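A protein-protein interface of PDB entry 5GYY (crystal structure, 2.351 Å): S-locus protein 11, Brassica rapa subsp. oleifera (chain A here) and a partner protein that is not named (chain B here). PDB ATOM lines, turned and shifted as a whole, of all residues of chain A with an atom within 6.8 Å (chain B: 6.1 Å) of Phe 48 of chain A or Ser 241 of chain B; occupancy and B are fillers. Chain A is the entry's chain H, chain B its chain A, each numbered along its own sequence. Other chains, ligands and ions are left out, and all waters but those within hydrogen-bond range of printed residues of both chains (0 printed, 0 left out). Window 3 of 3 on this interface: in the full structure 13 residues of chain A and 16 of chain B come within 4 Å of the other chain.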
ATOM      1  N   GLY A  16      34.615   1.389 -13.190  1.00  0.00           N
ATOM      2  CA  GLY A  16      33.905   2.508 -12.603  1.00  0.00           C
ATOM      3  C   GLY A  16      34.153   3.789 -13.368  1.00  0.00           C
ATOM      4  O   GLY A  16      35.231   3.992 -13.927  1.00  0.00           O
ATOM      5  N   GLY A  17      33.152   4.660 -13.391  1.00  0.00           N
ATOM      6  CA  GLY A  17      33.290   5.943 -14.068  1.00  0.00           C
ATOM      7  C   GLY A  17      32.336   6.121 -15.235  1.00  0.00           C
ATOM      8  O   GLY A  17      31.244   5.560 -15.259  1.00  0.00           O
ATOM      9  N   SER A  46      27.564   3.832 -20.785  1.00  0.00           N
ATOM     10  CA  SER A  46      27.930   4.270 -19.440  1.00  0.00           C
ATOM     11  C   SER A  46      26.829   4.350 -18.356  1.00  0.00           C
ATOM     12  O   SER A  46      26.864   5.254 -17.505  1.00  0.00           O
ATOM     13  CB  SER A  46      28.578   5.656 -19.612  1.00  0.00           C
ATOM     14  OG  SER A  46      29.168   6.111 -18.429  1.00  0.00           O
ATOM     15  N   PRO A  47      25.854   3.425 -18.355  1.00  0.00           N
ATOM     16  CA  PRO A  47      24.859   3.588 -17.288  1.00  0.00           C
ATOM     17  C   PRO A  47      25.420   2.992 -16.002  1.00  0.00           C
ATOM     18  O   PRO A  47      26.486   2.349 -16.043  1.00  0.00           O
ATOM     19  CB  PRO A  47      23.710   2.706 -17.770  1.00  0.00           C
ATOM     20  CG  PRO A  47      24.444   1.535 -18.377  1.00  0.00           C
ATOM     21  CD  PRO A  47      25.645   2.160 -19.090  1.00  0.00           C
ATOM     22  N   PHE A  48      24.708   3.172 -14.894  1.00  0.00           N
ATOM     23  CA  PHE A  48      25.100   2.592 -13.595  1.00  0.00           C
ATOM     24  C   PHE A  48      26.489   2.994 -13.090  1.00  0.00           C
ATOM     25  O   PHE A  48      27.208   2.153 -12.535  1.00  0.00           O
ATOM     26  CB  PHE A  48      25.034   1.062 -13.628  1.00  0.00           C
ATOM     27  CG  PHE A  48      23.751   0.511 -14.179  1.00  0.00           C
ATOM     28  CD1 PHE A  48      22.545   1.161 -13.959  1.00  0.00           C
ATOM     29  CD2 PHE A  48      23.750  -0.696 -14.871  1.00  0.00           C
ATOM     30  CE1 PHE A  48      21.349   0.648 -14.461  1.00  0.00           C
ATOM     31  CE2 PHE A  48      22.566  -1.228 -15.371  1.00  0.00           C
ATOM     32  CZ  PHE A  48      21.358  -0.550 -15.166  1.00  0.00           C
ATOM     33  N   ARG A  49      26.881   4.249 -13.309  1.00  0.00           N
ATOM     34  CA  ARG A  49      28.183   4.753 -12.842  1.00  0.00           C
ATOM     35  C   ARG A  49      29.359   3.859 -13.239  1.00  0.00           C
ATOM     36  O   ARG A  49      30.358   3.762 -12.518  1.00  0.00           O
ATOM     37  CB  ARG A  49      28.185   4.981 -11.323  1.00  0.00           C
ATOM     38  CG  ARG A  49      29.284   5.953 -10.856  1.00  0.00           C
ATOM     39  CD  ARG A  49      29.392   6.080  -9.322  1.00  0.00           C
ATOM     40  NE  ARG A  49      29.852   4.884  -8.604  1.00  0.00           N
ATOM     41  CZ  ARG A  49      31.008   4.251  -8.807  1.00  0.00           C
ATOM     42  NH1 ARG A  49      31.856   4.687  -9.715  1.00  0.00           N
ATOM     43  NH2 ARG A  49      31.315   3.176  -8.096  1.00  0.00           N
ATOM     44  N   THR A  50      29.236   3.225 -14.400  1.00  0.00           N
ATOM     45  CA  THR A  50      30.214   2.258 -14.876  1.00  0.00           C
ATOM     46  C   THR A  50      30.476   2.510 -16.365  1.00  0.00           C
ATOM     47  O   THR A  50      29.537   2.739 -17.125  1.00  0.00           O
ATOM     48  CB  THR A  50      29.646   0.836 -14.690  1.00  0.00           C
ATOM     49  OG1 THR A  50      29.265   0.661 -13.326  1.00  0.00           O
ATOM     50  CG2 THR A  50      30.643  -0.249 -15.114  1.00  0.00           C
ATOM     51  N   ARG A  51      31.741   2.476 -16.782  1.00  0.00           N
ATOM     52  CA  ARG A  51      32.070   2.548 -18.208  1.00  0.00           C
ATOM     53  C   ARG A  51      32.155   1.142 -18.835  1.00  0.00           C
ATOM     54  O   ARG A  51      32.976   0.318 -18.426  1.00  0.00           O
ATOM     55  CB  ARG A  51      33.401   3.280 -18.438  1.00  0.00           C
ATOM     56  CG  ARG A  51      33.666   3.586 -19.923  1.00  0.00           C
ATOM     57  CD  ARG A  51      35.072   4.115 -20.205  1.00  0.00           C
ATOM     58  NE  ARG A  51      36.163   3.237 -19.764  1.00  0.00           N
ATOM     59  CZ  ARG A  51      37.445   3.588 -19.810  1.00  0.00           C
ATOM     60  NH1 ARG A  51      37.783   4.784 -20.269  1.00  0.00           N
ATOM     61  NH2 ARG A  51      38.390   2.765 -19.392  1.00  0.00           N
ATOM     62  N   TYR A  52      31.300   0.871 -19.818  1.00  0.00           N
ATOM     63  CA  TYR A  52      31.342  -0.415 -20.509  1.00  0.00           C
ATOM     64  C   TYR A  52      31.964  -0.278 -21.899  1.00  0.00           C
ATOM     65  O   TYR A  52      31.349   0.274 -22.814  1.00  0.00           O
ATOM     66  CB  TYR A  52      29.943  -1.017 -20.652  1.00  0.00           C
ATOM     67  CG  TYR A  52      29.213  -1.294 -19.354  1.00  0.00           C
ATOM     68  CD1 TYR A  52      29.234  -2.556 -18.777  1.00  0.00           C
ATOM     69  CD2 TYR A  52      28.486  -0.295 -18.720  1.00  0.00           C
ATOM     70  CE1 TYR A  52      28.557  -2.817 -17.607  1.00  0.00           C
ATOM     71  CE2 TYR A  52      27.804  -0.539 -17.558  1.00  0.00           C
ATOM     72  CZ  TYR A  52      27.836  -1.802 -16.994  1.00  0.00           C
ATOM     73  OH  TYR A  52      27.155  -2.038 -15.810  1.00  0.00           O
ATOM     74  N   SER B 153      12.532  -1.613 -22.033  1.00  0.00           N
ATOM     75  CA  SER B 153      12.117  -0.404 -21.324  1.00  0.00           C
ATOM     76  C   SER B 153      11.590   0.684 -22.267  1.00  0.00           C
ATOM     77  O   SER B 153      11.897   0.686 -23.452  1.00  0.00           O
ATOM     78  CB  SER B 153      13.286   0.160 -20.527  1.00  0.00           C
ATOM     79  OG  SER B 153      14.332   0.534 -21.407  1.00  0.00           O
ATOM     80  N   TRP B 154      10.785   1.596 -21.725  1.00  0.00           N
ATOM     81  CA  TRP B 154      10.467   2.843 -22.402  1.00  0.00           C
ATOM     82  C   TRP B 154      11.759   3.626 -22.628  1.00  0.00           C
ATOM     83  O   TRP B 154      12.697   3.568 -21.825  1.00  0.00           O
ATOM     84  CB  TRP B 154       9.497   3.683 -21.572  1.00  0.00           C
ATOM     85  CG  TRP B 154       8.087   3.184 -21.528  1.00  0.00           C
ATOM     86  CD1 TRP B 154       7.662   1.874 -21.579  1.00  0.00           C
ATOM     87  CD2 TRP B 154       6.898   3.983 -21.428  1.00  0.00           C
ATOM     88  NE1 TRP B 154       6.286   1.818 -21.509  1.00  0.00           N
ATOM     89  CE2 TRP B 154       5.792   3.095 -21.420  1.00  0.00           C
ATOM     90  CE3 TRP B 154       6.660   5.364 -21.330  1.00  0.00           C
ATOM     91  CZ2 TRP B 154       4.468   3.546 -21.323  1.00  0.00           C
ATOM     92  CZ3 TRP B 154       5.343   5.810 -21.220  1.00  0.00           C
ATOM     93  CH2 TRP B 154       4.260   4.906 -21.228  1.00  0.00           C
ATOM     94  N   PHE B 165      17.204  -0.510 -22.771  1.00  0.00           N
ATOM     95  CA  PHE B 165      17.339  -1.597 -21.810  1.00  0.00           C
ATOM     96  C   PHE B 165      16.395  -2.769 -22.052  1.00  0.00           C
ATOM     97  O   PHE B 165      15.195  -2.598 -22.286  1.00  0.00           O
ATOM     98  CB  PHE B 165      17.187  -1.059 -20.385  1.00  0.00           C
ATOM     99  CG  PHE B 165      18.245  -0.073 -20.014  1.00  0.00           C
ATOM    100  CD1 PHE B 165      19.484  -0.504 -19.572  1.00  0.00           C
ATOM    101  CD2 PHE B 165      18.010   1.284 -20.118  1.00  0.00           C
ATOM    102  CE1 PHE B 165      20.471   0.406 -19.232  1.00  0.00           C
ATOM    103  CE2 PHE B 165      18.994   2.208 -19.777  1.00  0.00           C
ATOM    104  CZ  PHE B 165      20.224   1.766 -19.339  1.00  0.00           C
ATOM    105  N   THR B 180      20.651  -8.091 -17.863  1.00  0.00           N
ATOM    106  CA  THR B 180      20.207  -6.784 -18.360  1.00  0.00           C
ATOM    107  C   THR B 180      21.150  -6.294 -19.460  1.00  0.00           C
ATOM    108  O   THR B 180      22.363  -6.202 -19.265  1.00  0.00           O
ATOM    109  CB  THR B 180      20.103  -5.723 -17.233  1.00  0.00           C
ATOM    110  OG1 THR B 180      19.129  -6.141 -16.271  1.00  0.00           O
ATOM    111  CG2 THR B 180      19.663  -4.349 -17.788  1.00  0.00           C
ATOM    112  N   VAL B 187      25.138  -5.462 -19.359  1.00  0.00           N
ATOM    113  CA  VAL B 187      25.433  -4.469 -18.301  1.00  0.00           C
ATOM    114  C   VAL B 187      25.264  -4.963 -16.884  1.00  0.00           C
ATOM    115  O   VAL B 187      25.958  -4.505 -15.984  1.00  0.00           O
ATOM    116  CB  VAL B 187      24.675  -3.120 -18.482  1.00  0.00           C
ATOM    117  CG1 VAL B 187      25.165  -2.403 -19.740  1.00  0.00           C
ATOM    118  CG2 VAL B 187      23.167  -3.325 -18.529  1.00  0.00           C
ATOM    119  N   HIS B 188      24.349  -5.903 -16.686  1.00  0.00           N
ATOM    120  CA  HIS B 188      24.165  -6.533 -15.379  1.00  0.00           C
ATOM    121  C   HIS B 188      23.681  -7.960 -15.530  1.00  0.00           C
ATOM    122  O   HIS B 188      22.920  -8.277 -16.433  1.00  0.00           O
ATOM    123  CB  HIS B 188      23.175  -5.749 -14.502  1.00  0.00           C
ATOM    124  CG  HIS B 188      22.874  -6.409 -13.192  1.00  0.00           C
ATOM    125  ND1 HIS B 188      21.685  -7.061 -12.941  1.00  0.00           N
ATOM    126  CD2 HIS B 188      23.615  -6.530 -12.061  1.00  0.00           C
ATOM    127  CE1 HIS B 188      21.707  -7.559 -11.713  1.00  0.00           C
ATOM    128  NE2 HIS B 188      22.864  -7.245 -11.157  1.00  0.00           N
ATOM    129  N   ILE B 238      11.056  -2.838 -15.852  1.00  0.00           N
ATOM    130  CA  ILE B 238      12.357  -2.229 -16.042  1.00  0.00           C
ATOM    131  C   ILE B 238      12.149  -0.819 -16.555  1.00  0.00           C
ATOM    132  O   ILE B 238      11.588  -0.623 -17.636  1.00  0.00           O
ATOM    133  CB  ILE B 238      13.340  -3.081 -16.900  1.00  0.00           C
ATOM    134  CG1 ILE B 238      14.697  -2.376 -16.951  1.00  0.00           C
ATOM    135  CG2 ILE B 238      12.768  -3.394 -18.316  1.00  0.00           C
ATOM    136  CD1 ILE B 238      15.843  -3.282 -17.288  1.00  0.00           C
ATOM    137  N   ASN B 239      12.568   0.164 -15.746  1.00  0.00           N
ATOM    138  CA  ASN B 239      12.318   1.570 -16.062  1.00  0.00           C
ATOM    139  C   ASN B 239      13.278   2.118 -17.104  1.00  0.00           C
ATOM    140  O   ASN B 239      14.225   1.421 -17.497  1.00  0.00           O
ATOM    141  CB  ASN B 239      12.264   2.460 -14.799  1.00  0.00           C
ATOM    142  CG  ASN B 239      13.619   2.612 -14.087  1.00  0.00           C
ATOM    143  OD1 ASN B 239      14.686   2.690 -14.709  1.00  0.00           O
ATOM    144  ND2 ASN B 239      13.564   2.669 -12.764  1.00  0.00           N
ATOM    145  N   PHE B 240      13.042   3.355 -17.549  1.00  0.00           N
ATOM    146  CA  PHE B 240      13.872   3.922 -18.611  1.00  0.00           C
ATOM    147  C   PHE B 240      15.352   4.040 -18.258  1.00  0.00           C
ATOM    148  O   PHE B 240      16.201   4.080 -19.146  1.00  0.00           O
ATOM    149  CB  PHE B 240      13.320   5.273 -19.142  1.00  0.00           C
ATOM    150  CG  PHE B 240      13.362   6.405 -18.140  1.00  0.00           C
ATOM    151  CD1 PHE B 240      14.486   7.201 -18.018  1.00  0.00           C
ATOM    152  CD2 PHE B 240      12.257   6.689 -17.346  1.00  0.00           C
ATOM    153  CE1 PHE B 240      14.523   8.259 -17.097  1.00  0.00           C
ATOM    154  CE2 PHE B 240      12.286   7.747 -16.420  1.00  0.00           C
ATOM    155  CZ  PHE B 240      13.420   8.522 -16.288  1.00  0.00           C
ATOM    156  N   SER B 241      15.670   4.091 -16.972  1.00  0.00           N
ATOM    157  CA  SER B 241      17.067   4.230 -16.562  1.00  0.00           C
ATOM    158  C   SER B 241      17.782   2.902 -16.461  1.00  0.00           C
ATOM    159  O   SER B 241      18.971   2.864 -16.152  1.00  0.00           O
ATOM    160  CB  SER B 241      17.182   4.979 -15.239  1.00  0.00           C
ATOM    161  OG  SER B 241      16.745   6.314 -15.385  1.00  0.00           O
ATOM    162  N   GLY B 242      17.053   1.823 -16.748  1.00  0.00           N
ATOM    163  CA  GLY B 242      17.615   0.491 -16.771  1.00  0.00           C
ATOM    164  C   GLY B 242      17.523  -0.281 -15.459  1.00  0.00           C
ATOM    165  O   GLY B 242      18.224  -1.265 -15.275  1.00  0.00           O
ATOM    166  N   PHE B 243      16.693   0.160 -14.524  1.00  0.00           N
ATOM    167  CA  PHE B 243      16.542  -0.617 -13.310  1.00  0.00           C
ATOM    168  C   PHE B 243      15.306  -1.492 -13.410  1.00  0.00           C
ATOM    169  O   PHE B 243      14.206  -1.008 -13.672  1.00  0.00           O
ATOM    170  CB  PHE B 243      16.475   0.269 -12.053  1.00  0.00           C
ATOM    171  CG  PHE B 243      17.700   1.127 -11.835  1.00  0.00           C
ATOM    172  CD1 PHE B 243      18.783   0.653 -11.130  1.00  0.00           C
ATOM    173  CD2 PHE B 243      17.753   2.422 -12.342  1.00  0.00           C
ATOM    174  CE1 PHE B 243      19.901   1.466 -10.913  1.00  0.00           C
ATOM    175  CE2 PHE B 243      18.868   3.227 -12.144  1.00  0.00           C
ATOM    176  CZ  PHE B 243      19.946   2.745 -11.425  1.00  0.00           C
ATOM    177  N   SER B 262      17.173  -3.292  -9.048  1.00  0.00           N
ATOM    178  CA  SER B 262      18.365  -3.982  -9.517  1.00  0.00           C
ATOM    179  C   SER B 262      18.816  -3.345 -10.828  1.00  0.00           C
ATOM    180  O   SER B 262      17.988  -3.133 -11.722  1.00  0.00           O
ATOM    181  CB  SER B 262      18.080  -5.480  -9.709  1.00  0.00           C
ATOM    182  OG  SER B 262      19.266  -6.197 -10.024  1.00  0.00           O
ATOM    183  N   PRO B 263      20.121  -3.029 -10.944  1.00  0.00           N
ATOM    184  CA  PRO B 263      21.182  -3.261  -9.950  1.00  0.00           C
ATOM    185  C   PRO B 263      21.056  -2.374  -8.718  1.00  0.00           C
ATOM    186  O   PRO B 263      20.763  -1.185  -8.846  1.00  0.00           O
ATOM    187  CB  PRO B 263      22.467  -2.900 -10.705  1.00  0.00           C
ATOM    188  CG  PRO B 263      22.046  -2.067 -11.826  1.00  0.00           C
ATOM    189  CD  PRO B 263      20.656  -2.469 -12.193  1.00  0.00           C
ATOM    190  N   PHE B 266      25.901   0.402  -7.490  1.00  0.00           N
ATOM    191  CA  PHE B 266      26.773   0.786  -8.596  1.00  0.00           C
ATOM    192  C   PHE B 266      28.187   0.318  -8.313  1.00  0.00           C
ATOM    193  O   PHE B 266      29.005   0.201  -9.229  1.00  0.00           O
ATOM    194  CB  PHE B 266      26.787   2.297  -8.794  1.00  0.00           C
ATOM    195  CG  PHE B 266      25.516   2.852  -9.389  1.00  0.00           C
ATOM    196  CD1 PHE B 266      24.598   2.019 -10.017  1.00  0.00           C
ATOM    197  CD2 PHE B 266      25.258   4.221  -9.357  1.00  0.00           C
ATOM    198  CE1 PHE B 266      23.430   2.538 -10.562  1.00  0.00           C
ATOM    199  CE2 PHE B 266      24.097   4.739  -9.911  1.00  0.00           C
ATOM    200  CZ  PHE B 266      23.185   3.897 -10.512  1.00  0.00           C
ATOM    201  N   GLN B 267      28.478   0.082  -7.035  1.00  0.00           N
ATOM    202  CA  GLN B 267      29.800  -0.374  -6.616  1.00  0.00           C
ATOM    203  C   GLN B 267      30.094  -1.822  -7.036  1.00  0.00           C
ATOM    204  O   GLN B 267      31.152  -2.088  -7.595  1.00  0.00           O
ATOM    205  CB  GLN B 267      29.974  -0.264  -5.096  1.00  0.00           C
ATOM    206  CG  GLN B 267      29.979   1.161  -4.532  1.00  0.00           C
ATOM    207  CD  GLN B 267      28.580   1.722  -4.346  1.00  0.00           C
ATOM    208  OE1 GLN B 267      27.598   0.980  -4.314  1.00  0.00           O
ATOM    209  NE2 GLN B 267      28.488   3.034  -4.196  1.00  0.00           N
ATOM    210  N   PRO B 270      27.397  -3.983 -11.121  1.00  0.00           N
ATOM    211  CA  PRO B 270      27.663  -4.000 -12.570  1.00  0.00           C
ATOM    212  C   PRO B 270      28.489  -5.199 -13.075  1.00  0.00           C
ATOM    213  O   PRO B 270      29.387  -5.701 -12.405  1.00  0.00           O
ATOM    214  CB  PRO B 270      28.404  -2.677 -12.801  1.00  0.00           C
ATOM    215  CG  PRO B 270      27.836  -1.775 -11.784  1.00  0.00           C
ATOM    216  CD  PRO B 270      27.592  -2.633 -10.559  1.00  0.00           C
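Phe 48 of chain A touches six residues of chain B.
Of chain A, only Phe 48 (3.7 Å) comes within 4 Å of Ser 241 of chain B.
Of the printed residues of chain B, Thr 50 of chain A touches Pro 270.
Of the printed residues of chain A, Phe 266 of chain B touches Phe 48 (3.5 Å) and Arg 49 (3.6 Å).
Ser 46 of chain A touches none of the printed residues of chain B.
The nearest residue of chain A that does not touch Ser 241 of chain B is Pro 47 of chain A (5.0 Å).
Among the printed residues, pairs that only touch across the chains: Pro 47 of chain A with Phe 165 of chain B (3.9 Å), Phe 48 of chain A with Val 187 of chain B (3.8 Å), Phe 48 of chain A with Ser 241 of chain B (3.7 Å), Phe 48 of chain A with Gly 242 of chain B (3.2 Å), Phe 48 of chain A with Phe 243 of chain B (3.9 Å), Phe 48 of chain A with Pro 263 of chain B (3.6 Å), Phe 48 of chain A with Phe 266 of chain B (3.5 Å), Arg 49 of chain A with Phe 266 of chain B (3.6 Å), Thr 50 of chain A with Pro 270 of chain B (3.2 Å) and Tyr 52 of chain A with Pro 270 of chain B (3.3 Å).
Hydrophobic or aromatic side chains of chain A that line the printed part of chain B: Pro 47, Phe 48 and Tyr 52.
Hydrophobic or aromatic side chains of chain B that line the printed part of chain A: Phe 165, Val 187, Phe 243, Pro 263, Phe 266 and Pro 270.
Along chain B the printed residues that touch a printed residue of chain A span positions 165 to 270.
Among the printed residues, 11 pairs touch across the chains.
Among the printed residues, no Asp or Glu carboxylate lies within 4 Å of a Lys or Arg side-chain nitrogen of the other chain.
N of Phe 243 of chain B sits at hydrogen-bond distance from OD1 of Asn 239 of chain B (3.2 Å).
The backbone NH (N) of Ser 153 of chain B is in hydrogen-bond range of the backbone carbonyl oxygen (O) of Phe 165 of chain B (2.9 Å).
The backbone NH of Ser 241 of chain B lies within hydrogen-bond range of the side-chain amide oxygen of Asn 239 of chain B, at 2.8 Å.
The backbone carbonyl oxygen (O) of Arg 49 of chain A sits at hydrogen-bond distance from the backbone NH (N) of Gly 17 of chain A, 3.1 Å away.
The backbone NH (N) of Val 187 of chain B is in hydrogen-bond range of the backbone carbonyl oxygen (O) of Thr 180 of chain B (2.9 Å).
OG1 of Thr 50 of chain A is in hydrogen-bond range of O of Phe 48 of chain A, 2.7 Å away.
The backbone carbonyl oxygen (O) of Val 187 of chain B lies within hydrogen-bond range of the side-chain hydroxyl (OH) of Tyr 52 of chain A, at 2.7 Å.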
